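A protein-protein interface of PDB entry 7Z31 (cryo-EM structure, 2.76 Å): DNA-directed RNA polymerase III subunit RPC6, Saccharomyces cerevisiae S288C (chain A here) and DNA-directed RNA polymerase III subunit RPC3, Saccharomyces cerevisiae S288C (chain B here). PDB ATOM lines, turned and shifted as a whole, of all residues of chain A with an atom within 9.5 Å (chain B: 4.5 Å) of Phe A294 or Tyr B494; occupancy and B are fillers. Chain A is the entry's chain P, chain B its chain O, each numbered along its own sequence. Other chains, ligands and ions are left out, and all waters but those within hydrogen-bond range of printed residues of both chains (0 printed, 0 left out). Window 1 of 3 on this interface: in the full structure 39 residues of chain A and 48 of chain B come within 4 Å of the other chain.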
ATOM      1  N   ASP A 250      -3.619  33.638 -34.146  1.00  0.00           N
ATOM      2  CA  ASP A 250      -4.424  33.965 -32.970  1.00  0.00           C
ATOM      3  C   ASP A 250      -5.745  33.200 -32.933  1.00  0.00           C
ATOM      4  O   ASP A 250      -6.628  33.539 -32.136  1.00  0.00           O
ATOM      5  CB  ASP A 250      -4.698  35.474 -32.861  1.00  0.00           C
ATOM      6  CG  ASP A 250      -4.434  36.017 -31.477  1.00  0.00           C
ATOM      7  OD1 ASP A 250      -3.605  35.433 -30.750  1.00  0.00           O
ATOM      8  OD2 ASP A 250      -5.061  37.035 -31.113  1.00  0.00           O
ATOM      9  N   ASP A 251      -5.896  32.177 -33.777  1.00  0.00           N
ATOM     10  CA  ASP A 251      -7.083  31.317 -33.811  1.00  0.00           C
ATOM     11  C   ASP A 251      -8.362  32.132 -34.013  1.00  0.00           C
ATOM     12  O   ASP A 251      -9.375  31.929 -33.338  1.00  0.00           O
ATOM     13  CB  ASP A 251      -7.167  30.459 -32.547  1.00  0.00           C
ATOM     14  CG  ASP A 251      -8.030  29.221 -32.731  1.00  0.00           C
ATOM     15  OD1 ASP A 251      -8.152  28.731 -33.875  1.00  0.00           O
ATOM     16  OD2 ASP A 251      -8.596  28.740 -31.727  1.00  0.00           O
ATOM     17  N   LYS A 252      -8.310  33.066 -34.967  1.00  0.00           N
ATOM     18  CA  LYS A 252      -9.442  33.948 -35.237  1.00  0.00           C
ATOM     19  C   LYS A 252     -10.337  33.434 -36.362  1.00  0.00           C
ATOM     20  O   LYS A 252     -11.503  33.832 -36.453  1.00  0.00           O
ATOM     21  CB  LYS A 252      -8.945  35.357 -35.576  1.00  0.00           C
ATOM     22  CG  LYS A 252      -8.069  35.994 -34.507  1.00  0.00           C
ATOM     23  CD  LYS A 252      -8.907  36.677 -33.442  1.00  0.00           C
ATOM     24  CE  LYS A 252      -8.062  37.082 -32.254  1.00  0.00           C
ATOM     25  NZ  LYS A 252      -7.585  35.888 -31.498  1.00  0.00           N
ATOM     26  N   THR A 264     -14.796  29.903 -34.559  1.00  0.00           N
ATOM     27  CA  THR A 264     -15.150  28.754 -33.730  1.00  0.00           C
ATOM     28  C   THR A 264     -15.702  29.163 -32.371  1.00  0.00           C
ATOM     29  O   THR A 264     -16.825  28.778 -32.032  1.00  0.00           O
ATOM     30  CB  THR A 264     -13.936  27.830 -33.555  1.00  0.00           C
ATOM     31  OG1 THR A 264     -13.039  28.391 -32.590  1.00  0.00           O
ATOM     32  CG2 THR A 264     -13.198  27.658 -34.879  1.00  0.00           C
ATOM     33  N   LEU A 265     -14.957  29.942 -31.581  1.00  0.00           N
ATOM     34  CA  LEU A 265     -15.322  30.247 -30.201  1.00  0.00           C
ATOM     35  C   LEU A 265     -15.142  31.727 -29.885  1.00  0.00           C
ATOM     36  O   LEU A 265     -14.788  32.087 -28.758  1.00  0.00           O
ATOM     37  CB  LEU A 265     -14.511  29.391 -29.226  1.00  0.00           C
ATOM     38  CG  LEU A 265     -13.006  29.233 -29.489  1.00  0.00           C
ATOM     39  CD1 LEU A 265     -12.189  30.441 -29.050  1.00  0.00           C
ATOM     40  CD2 LEU A 265     -12.460  27.968 -28.842  1.00  0.00           C
ATOM     41  N   GLU A 266     -15.386  32.596 -30.868  1.00  0.00           N
ATOM     42  CA  GLU A 266     -15.067  34.009 -30.698  1.00  0.00           C
ATOM     43  C   GLU A 266     -15.903  34.647 -29.596  1.00  0.00           C
ATOM     44  O   GLU A 266     -15.383  35.425 -28.789  1.00  0.00           O
ATOM     45  CB  GLU A 266     -15.247  34.748 -32.020  1.00  0.00           C
ATOM     46  CG  GLU A 266     -14.069  34.575 -32.973  1.00  0.00           C
ATOM     47  CD  GLU A 266     -12.817  35.290 -32.493  1.00  0.00           C
ATOM     48  OE1 GLU A 266     -12.926  36.171 -31.611  1.00  0.00           O
ATOM     49  OE2 GLU A 266     -11.719  34.975 -32.999  1.00  0.00           O
ATOM     50  N   ILE A 268     -17.234  33.171 -26.960  1.00  0.00           N
ATOM     51  CA  ILE A 268     -16.781  32.676 -25.663  1.00  0.00           C
ATOM     52  C   ILE A 268     -15.467  33.336 -25.263  1.00  0.00           C
ATOM     53  O   ILE A 268     -15.284  33.732 -24.105  1.00  0.00           O
ATOM     54  CB  ILE A 268     -16.674  31.142 -25.689  1.00  0.00           C
ATOM     55  CG1 ILE A 268     -18.070  30.532 -25.854  1.00  0.00           C
ATOM     56  CG2 ILE A 268     -16.004  30.625 -24.424  1.00  0.00           C
ATOM     57  CD1 ILE A 268     -18.079  29.040 -26.032  1.00  0.00           C
ATOM     58  N   LEU A 269     -14.533  33.476 -26.210  1.00  0.00           N
ATOM     59  CA  LEU A 269     -13.253  34.093 -25.870  1.00  0.00           C
ATOM     60  C   LEU A 269     -13.424  35.567 -25.521  1.00  0.00           C
ATOM     61  O   LEU A 269     -12.772  36.071 -24.597  1.00  0.00           O
ATOM     62  CB  LEU A 269     -12.246  33.906 -27.011  1.00  0.00           C
ATOM     63  CG  LEU A 269     -12.285  34.738 -28.297  1.00  0.00           C
ATOM     64  CD1 LEU A 269     -11.518  36.045 -28.142  1.00  0.00           C
ATOM     65  CD2 LEU A 269     -11.719  33.938 -29.459  1.00  0.00           C
ATOM     66  N   GLN A 270     -14.292  36.279 -26.247  1.00  0.00           N
ATOM     67  CA  GLN A 270     -14.554  37.677 -25.926  1.00  0.00           C
ATOM     68  C   GLN A 270     -15.231  37.812 -24.571  1.00  0.00           C
ATOM     69  O   GLN A 270     -14.931  38.736 -23.807  1.00  0.00           O
ATOM     70  CB  GLN A 270     -15.406  38.316 -27.023  1.00  0.00           C
ATOM     71  CG  GLN A 270     -14.660  38.548 -28.320  1.00  0.00           C
ATOM     72  CD  GLN A 270     -13.510  39.517 -28.158  1.00  0.00           C
ATOM     73  OE1 GLN A 270     -12.386  39.119 -27.847  1.00  0.00           O
ATOM     74  NE2 GLN A 270     -13.782  40.799 -28.367  1.00  0.00           N
ATOM     75  N   PHE A 291     -10.224  19.973 -18.794  1.00  0.00           N
ATOM     76  CA  PHE A 291     -10.017  21.326 -18.293  1.00  0.00           C
ATOM     77  C   PHE A 291     -10.522  22.384 -19.269  1.00  0.00           C
ATOM     78  O   PHE A 291     -10.829  23.511 -18.870  1.00  0.00           O
ATOM     79  CB  PHE A 291      -8.537  21.566 -17.997  1.00  0.00           C
ATOM     80  CG  PHE A 291      -8.182  23.020 -17.831  1.00  0.00           C
ATOM     81  CD1 PHE A 291      -8.606  23.729 -16.720  1.00  0.00           C
ATOM     82  CD2 PHE A 291      -7.441  23.681 -18.796  1.00  0.00           C
ATOM     83  CE1 PHE A 291      -8.289  25.068 -16.569  1.00  0.00           C
ATOM     84  CE2 PHE A 291      -7.120  25.018 -18.649  1.00  0.00           C
ATOM     85  CZ  PHE A 291      -7.544  25.710 -17.533  1.00  0.00           C
ATOM     86  N   SER A 292     -10.635  22.001 -20.543  1.00  0.00           N
ATOM     87  CA  SER A 292     -10.899  22.928 -21.642  1.00  0.00           C
ATOM     88  C   SER A 292      -9.776  23.967 -21.748  1.00  0.00           C
ATOM     89  O   SER A 292      -9.953  25.165 -21.510  1.00  0.00           O
ATOM     90  CB  SER A 292     -12.271  23.597 -21.490  1.00  0.00           C
ATOM     91  OG  SER A 292     -12.238  24.620 -20.513  1.00  0.00           O
ATOM     92  N   ILE A 293      -8.597  23.449 -22.105  1.00  0.00           N
ATOM     93  CA  ILE A 293      -7.391  24.244 -22.300  1.00  0.00           C
ATOM     94  C   ILE A 293      -7.555  25.331 -23.353  1.00  0.00           C
ATOM     95  O   ILE A 293      -6.659  26.164 -23.524  1.00  0.00           O
ATOM     96  CB  ILE A 293      -6.220  23.318 -22.690  1.00  0.00           C
ATOM     97  CG1 ILE A 293      -6.418  21.934 -22.075  1.00  0.00           C
ATOM     98  CG2 ILE A 293      -4.880  23.913 -22.269  1.00  0.00           C
ATOM     99  CD1 ILE A 293      -5.500  20.884 -22.648  1.00  0.00           C
ATOM    100  N   PHE A 294      -8.673  25.341 -24.070  1.00  0.00           N
ATOM    101  CA  PHE A 294      -8.893  26.275 -25.161  1.00  0.00           C
ATOM    102  C   PHE A 294      -9.642  27.531 -24.731  1.00  0.00           C
ATOM    103  O   PHE A 294     -10.075  28.300 -25.594  1.00  0.00           O
ATOM    104  CB  PHE A 294      -9.638  25.570 -26.298  1.00  0.00           C
ATOM    105  CG  PHE A 294      -8.978  24.289 -26.749  1.00  0.00           C
ATOM    106  CD1 PHE A 294      -9.264  23.087 -26.120  1.00  0.00           C
ATOM    107  CD2 PHE A 294      -8.071  24.290 -27.799  1.00  0.00           C
ATOM    108  CE1 PHE A 294      -8.660  21.915 -26.529  1.00  0.00           C
ATOM    109  CE2 PHE A 294      -7.466  23.122 -28.211  1.00  0.00           C
ATOM    110  CZ  PHE A 294      -7.761  21.931 -27.578  1.00  0.00           C
ATOM    111  N   ASN A 295      -9.817  27.742 -23.426  1.00  0.00           N
ATOM    112  CA  ASN A 295     -10.430  28.955 -22.897  1.00  0.00           C
ATOM    113  C   ASN A 295     -10.155  29.011 -21.401  1.00  0.00           C
ATOM    114  O   ASN A 295     -10.471  28.061 -20.679  1.00  0.00           O
ATOM    115  CB  ASN A 295     -11.942  28.992 -23.175  1.00  0.00           C
ATOM    116  CG  ASN A 295     -12.663  27.751 -22.674  1.00  0.00           C
ATOM    117  OD1 ASN A 295     -12.073  26.679 -22.571  1.00  0.00           O
ATOM    118  ND2 ASN A 295     -13.953  27.891 -22.376  1.00  0.00           N
ATOM    119  N   TYR A 296      -9.571  30.120 -20.937  1.00  0.00           N
ATOM    120  CA  TYR A 296      -9.152  30.228 -19.544  1.00  0.00           C
ATOM    121  C   TYR A 296      -9.547  31.547 -18.889  1.00  0.00           C
ATOM    122  O   TYR A 296      -8.994  31.890 -17.836  1.00  0.00           O
ATOM    123  CB  TYR A 296      -7.635  30.027 -19.421  1.00  0.00           C
ATOM    124  CG  TYR A 296      -6.815  30.994 -20.239  1.00  0.00           C
ATOM    125  CD1 TYR A 296      -6.416  32.217 -19.712  1.00  0.00           C
ATOM    126  CD2 TYR A 296      -6.430  30.682 -21.539  1.00  0.00           C
ATOM    127  CE1 TYR A 296      -5.666  33.104 -20.457  1.00  0.00           C
ATOM    128  CE2 TYR A 296      -5.680  31.563 -22.292  1.00  0.00           C
ATOM    129  CZ  TYR A 296      -5.298  32.771 -21.746  1.00  0.00           C
ATOM    130  OH  TYR A 296      -4.547  33.653 -22.489  1.00  0.00           O
ATOM    131  N   PHE A 297     -10.468  32.306 -19.482  1.00  0.00           N
ATOM    132  CA  PHE A 297     -10.962  33.494 -18.801  1.00  0.00           C
ATOM    133  C   PHE A 297     -11.969  33.159 -17.708  1.00  0.00           C
ATOM    134  O   PHE A 297     -12.086  33.919 -16.742  1.00  0.00           O
ATOM    135  CB  PHE A 297     -11.565  34.475 -19.805  1.00  0.00           C
ATOM    136  CG  PHE A 297     -10.546  35.362 -20.462  1.00  0.00           C
ATOM    137  CD1 PHE A 297      -9.194  35.062 -20.382  1.00  0.00           C
ATOM    138  CD2 PHE A 297     -10.933  36.508 -21.138  1.00  0.00           C
ATOM    139  CE1 PHE A 297      -8.253  35.871 -20.979  1.00  0.00           C
ATOM    140  CE2 PHE A 297      -9.993  37.328 -21.735  1.00  0.00           C
ATOM    141  CZ  PHE A 297      -8.653  37.010 -21.657  1.00  0.00           C
ATOM    142  N   LYS A 298     -12.697  32.047 -17.835  1.00  0.00           N
ATOM    143  CA  LYS A 298     -13.580  31.626 -16.750  1.00  0.00           C
ATOM    144  C   LYS A 298     -12.800  31.285 -15.490  1.00  0.00           C
ATOM    145  O   LYS A 298     -13.196  31.685 -14.389  1.00  0.00           O
ATOM    146  CB  LYS A 298     -14.415  30.419 -17.176  1.00  0.00           C
ATOM    147  CG  LYS A 298     -15.860  30.732 -17.504  1.00  0.00           C
ATOM    148  CD  LYS A 298     -16.684  29.463 -17.578  1.00  0.00           C
ATOM    149  CE  LYS A 298     -16.690  28.727 -16.247  1.00  0.00           C
ATOM    150  NZ  LYS A 298     -17.124  29.598 -15.126  1.00  0.00           N
ATOM    151  N   MET A 299     -11.701  30.549 -15.629  1.00  0.00           N
ATOM    152  CA  MET A 299     -10.881  30.146 -14.496  1.00  0.00           C
ATOM    153  C   MET A 299      -9.931  31.285 -14.151  1.00  0.00           C
ATOM    154  O   MET A 299      -9.121  31.702 -14.985  1.00  0.00           O
ATOM    155  CB  MET A 299     -10.101  28.874 -14.822  1.00  0.00           C
ATOM    156  CG  MET A 299     -10.912  27.824 -15.559  1.00  0.00           C
ATOM    157  SD  MET A 299     -12.190  27.074 -14.537  1.00  0.00           S
ATOM    158  CE  MET A 299     -13.361  26.573 -15.793  1.00  0.00           C
ATOM    159  N   PHE A 312       4.994  27.795 -15.230  1.00  0.00           N
ATOM    160  CA  PHE A 312       5.437  27.130 -16.451  1.00  0.00           C
ATOM    161  C   PHE A 312       6.893  27.416 -16.787  1.00  0.00           C
ATOM    162  O   PHE A 312       7.584  26.534 -17.310  1.00  0.00           O
ATOM    163  CB  PHE A 312       4.544  27.541 -17.625  1.00  0.00           C
ATOM    164  CG  PHE A 312       5.063  27.116 -18.964  1.00  0.00           C
ATOM    165  CD1 PHE A 312       5.285  25.782 -19.246  1.00  0.00           C
ATOM    166  CD2 PHE A 312       5.319  28.054 -19.946  1.00  0.00           C
ATOM    167  CE1 PHE A 312       5.760  25.394 -20.480  1.00  0.00           C
ATOM    168  CE2 PHE A 312       5.788  27.671 -21.182  1.00  0.00           C
ATOM    169  CZ  PHE A 312       6.014  26.338 -21.449  1.00  0.00           C
ATOM    170  N   LEU B 299     -13.039  19.863 -25.632  1.00  0.00           N
ATOM    171  CA  LEU B 299     -12.686  20.674 -26.792  1.00  0.00           C
ATOM    172  C   LEU B 299     -13.937  21.117 -27.539  1.00  0.00           C
ATOM    173  O   LEU B 299     -14.074  22.289 -27.912  1.00  0.00           O
ATOM    174  CB  LEU B 299     -11.753  19.872 -27.705  1.00  0.00           C
ATOM    175  CG  LEU B 299     -11.278  20.397 -29.065  1.00  0.00           C
ATOM    176  CD1 LEU B 299      -9.955  19.751 -29.416  1.00  0.00           C
ATOM    177  CD2 LEU B 299     -12.277  20.115 -30.178  1.00  0.00           C
ATOM    178  N   THR B 302     -15.852  23.826 -25.608  1.00  0.00           N
ATOM    179  CA  THR B 302     -15.335  25.182 -25.775  1.00  0.00           C
ATOM    180  C   THR B 302     -15.621  25.734 -27.170  1.00  0.00           C
ATOM    181  O   THR B 302     -15.952  26.917 -27.318  1.00  0.00           O
ATOM    182  CB  THR B 302     -13.835  25.217 -25.489  1.00  0.00           C
ATOM    183  OG1 THR B 302     -13.599  24.836 -24.128  1.00  0.00           O
ATOM    184  CG2 THR B 302     -13.296  26.610 -25.710  1.00  0.00           C
ATOM    185  N   SER B 490      -2.695  21.494 -31.910  1.00  0.00           N
ATOM    186  CA  SER B 490      -3.633  22.471 -31.371  1.00  0.00           C
ATOM    187  C   SER B 490      -3.455  22.626 -29.866  1.00  0.00           C
ATOM    188  O   SER B 490      -3.449  23.748 -29.343  1.00  0.00           O
ATOM    189  CB  SER B 490      -5.068  22.061 -31.706  1.00  0.00           C
ATOM    190  OG  SER B 490      -5.364  20.758 -31.225  1.00  0.00           O
ATOM    191  N   VAL B 491      -3.300  21.507 -29.156  1.00  0.00           N
ATOM    192  CA  VAL B 491      -3.145  21.562 -27.704  1.00  0.00           C
ATOM    193  C   VAL B 491      -1.840  22.254 -27.334  1.00  0.00           C
ATOM    194  O   VAL B 491      -1.797  23.087 -26.424  1.00  0.00           O
ATOM    195  CB  VAL B 491      -3.234  20.152 -27.096  1.00  0.00           C
ATOM    196  CG1 VAL B 491      -3.065  20.218 -25.587  1.00  0.00           C
ATOM    197  CG2 VAL B 491      -4.570  19.515 -27.445  1.00  0.00           C
ATOM    198  N   TYR B 492      -0.755  21.918 -28.034  1.00  0.00           N
ATOM    199  CA  TYR B 492       0.535  22.553 -27.784  1.00  0.00           C
ATOM    200  C   TYR B 492       0.454  24.053 -28.029  1.00  0.00           C
ATOM    201  O   TYR B 492       0.930  24.859 -27.218  1.00  0.00           O
ATOM    202  CB  TYR B 492       1.601  21.906 -28.673  1.00  0.00           C
ATOM    203  CG  TYR B 492       3.006  22.440 -28.492  1.00  0.00           C
ATOM    204  CD1 TYR B 492       3.699  22.235 -27.309  1.00  0.00           C
ATOM    205  CD2 TYR B 492       3.650  23.118 -29.516  1.00  0.00           C
ATOM    206  CE1 TYR B 492       4.988  22.708 -27.146  1.00  0.00           C
ATOM    207  CE2 TYR B 492       4.941  23.593 -29.359  1.00  0.00           C
ATOM    208  CZ  TYR B 492       5.603  23.386 -28.168  1.00  0.00           C
ATOM    209  OH  TYR B 492       6.887  23.855 -27.990  1.00  0.00           O
ATOM    210  N   GLU B 493      -0.185  24.443 -29.134  1.00  0.00           N
ATOM    211  CA  GLU B 493      -0.322  25.855 -29.461  1.00  0.00           C
ATOM    212  C   GLU B 493      -1.122  26.596 -28.403  1.00  0.00           C
ATOM    213  O   GLU B 493      -0.734  27.689 -27.973  1.00  0.00           O
ATOM    214  CB  GLU B 493      -0.986  26.013 -30.827  1.00  0.00           C
ATOM    215  CG  GLU B 493      -1.020  27.448 -31.289  1.00  0.00           C
ATOM    216  CD  GLU B 493       0.364  27.991 -31.576  1.00  0.00           C
ATOM    217  OE1 GLU B 493       1.275  27.179 -31.856  1.00  0.00           O
ATOM    218  OE2 GLU B 493       0.544  29.226 -31.528  1.00  0.00           O
ATOM    219  N   TYR B 494      -2.238  26.018 -27.958  1.00  0.00           N
ATOM    220  CA  TYR B 494      -3.061  26.723 -26.988  1.00  0.00           C
ATOM    221  C   TYR B 494      -2.443  26.711 -25.598  1.00  0.00           C
ATOM    222  O   TYR B 494      -2.672  27.642 -24.827  1.00  0.00           O
ATOM    223  CB  TYR B 494      -4.477  26.146 -26.954  1.00  0.00           C
ATOM    224  CG  TYR B 494      -5.539  27.220 -26.820  1.00  0.00           C
ATOM    225  CD1 TYR B 494      -5.469  28.168 -25.808  1.00  0.00           C
ATOM    226  CD2 TYR B 494      -6.592  27.306 -27.726  1.00  0.00           C
ATOM    227  CE1 TYR B 494      -6.423  29.156 -25.683  1.00  0.00           C
ATOM    228  CE2 TYR B 494      -7.549  28.296 -27.614  1.00  0.00           C
ATOM    229  CZ  TYR B 494      -7.458  29.217 -26.587  1.00  0.00           C
ATOM    230  OH  TYR B 494      -8.408  30.203 -26.460  1.00  0.00           O
ATOM    231  N   VAL B 495      -1.652  25.695 -25.255  1.00  0.00           N
ATOM    232  CA  VAL B 495      -0.920  25.735 -23.992  1.00  0.00           C
ATOM    233  C   VAL B 495       0.110  26.855 -24.017  1.00  0.00           C
ATOM    234  O   VAL B 495       0.244  27.624 -23.055  1.00  0.00           O
ATOM    235  CB  VAL B 495      -0.264  24.376 -23.698  1.00  0.00           C
ATOM    236  CG1 VAL B 495       0.719  24.506 -22.546  1.00  0.00           C
ATOM    237  CG2 VAL B 495      -1.330  23.345 -23.373  1.00  0.00           C
ATOM    238  N   ILE B 496       0.850  26.971 -25.121  1.00  0.00           N
ATOM    239  CA  ILE B 496       1.815  28.061 -25.231  1.00  0.00           C
ATOM    240  C   ILE B 496       1.098  29.405 -25.185  1.00  0.00           C
ATOM    241  O   ILE B 496       1.570  30.353 -24.551  1.00  0.00           O
ATOM    242  CB  ILE B 496       2.672  27.903 -26.503  1.00  0.00           C
ATOM    243  CG1 ILE B 496       3.939  27.101 -26.196  1.00  0.00           C
ATOM    244  CG2 ILE B 496       3.040  29.258 -27.085  1.00  0.00           C
ATOM    245  CD1 ILE B 496       3.687  25.655 -25.805  1.00  0.00           C
ATOM    246  N   ALA B 497      -0.072  29.496 -25.825  1.00  0.00           N
ATOM    247  CA  ALA B 497      -0.824  30.747 -25.842  1.00  0.00           C
ATOM    248  C   ALA B 497      -1.401  31.083 -24.472  1.00  0.00           C
ATOM    249  O   ALA B 497      -1.524  32.258 -24.120  1.00  0.00           O
ATOM    250  CB  ALA B 497      -1.936  30.669 -26.885  1.00  0.00           C
ATOM    251  N   SER B 498      -1.805  30.069 -23.705  1.00  0.00           N
ATOM    252  CA  SER B 498      -2.302  30.304 -22.354  1.00  0.00           C
ATOM    253  C   SER B 498      -1.175  30.746 -21.432  1.00  0.00           C
ATOM    254  O   SER B 498      -1.364  31.625 -20.583  1.00  0.00           O
ATOM    255  CB  SER B 498      -2.977  29.039 -21.819  1.00  0.00           C
ATOM    256  OG  SER B 498      -3.336  29.173 -20.453  1.00  0.00           O
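Hydrophobic or aromatic side chains of chain A that line the printed part of chain B: Leu A265, Ile A268, Ile A293, Phe A294 and Tyr A296.
Along chain A the printed residues that touch a printed residue of chain B span positions 265 to 296.
Among the printed residues, 12 pairs touch across the chains.
Among the printed residues, no Asp or Glu carboxylate lies within 4 Å of a Lys or Arg side-chain nitrogen of the other chain.
Among the printed residues, merely in contact across the chains: Ser A292 with Thr B302 (3.2 Å), Ile A293 with Tyr B494 (3.3 Å), Ile A268 with Thr B302 (3.3 Å), Leu A265 with Thr B302 (3.4 Å), Phe A294 with Leu B299 (3.6 Å), Tyr A296 with Ser B498 (3.6 Å), Phe A294 with Thr B302 (3.6 Å), Tyr A296 with Ala B497 (3.7 Å), Ile A293 with Val B495 (3.8 Å) and Ile A293 with Val B491 (3.9 Å).
The backbone carbonyl oxygen (O) of Ser A292 lies close to the side-chain amide oxygen (OD1) of Asn A295.
OG1 of Thr B302 is in hydrogen-bond range of OD1 of Asn A295 (2.9 Å).
The side-chain hydroxyl (OH) of Tyr B494 is in hydrogen-bond range of the backbone carbonyl oxygen (O) of Phe A294 (2.7 Å).
Of the printed residues of chain B, Phe A294 touches Leu B299, Thr B302 and Tyr B494.
Printed residues of chain A within 4 Å of Tyr B494: Ile A293 (3.3 Å) and Phe A294 (2.7 Å).
Of the printed residues of chain A, Val B495 touches Ile A293 (3.8 Å).
Ala B497 touches just one residue of chain A: Tyr A296.
Of the printed residues of chain A, Val B491 touches Ile A293 (3.9 Å).
Printed residues of chain B within 4 Å of Leu A265: Thr B302.
Of the printed residues of chain A, Thr B302 touches Leu A265 (3.4 Å), Ile A268 (3.3 Å), Ser A292 (3.2 Å), Phe A294 (3.6 Å) and Asn A295 (2.9 Å).
Of the printed residues of chain B, Tyr A296 touches Ala B497 and Ser B498.
Asp A250 touches none of the printed residues of chain B.
The nearest printed residue of chain B that does not touch Phe A294 is Val B491 (4.005 Å).
The nearest residue of chain A that does not touch Tyr B494 is Asn A295 (4.2 Å).
The nearest printed residue of chain B that does not touch Ser A292 is Leu B299 (5.5 Å).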
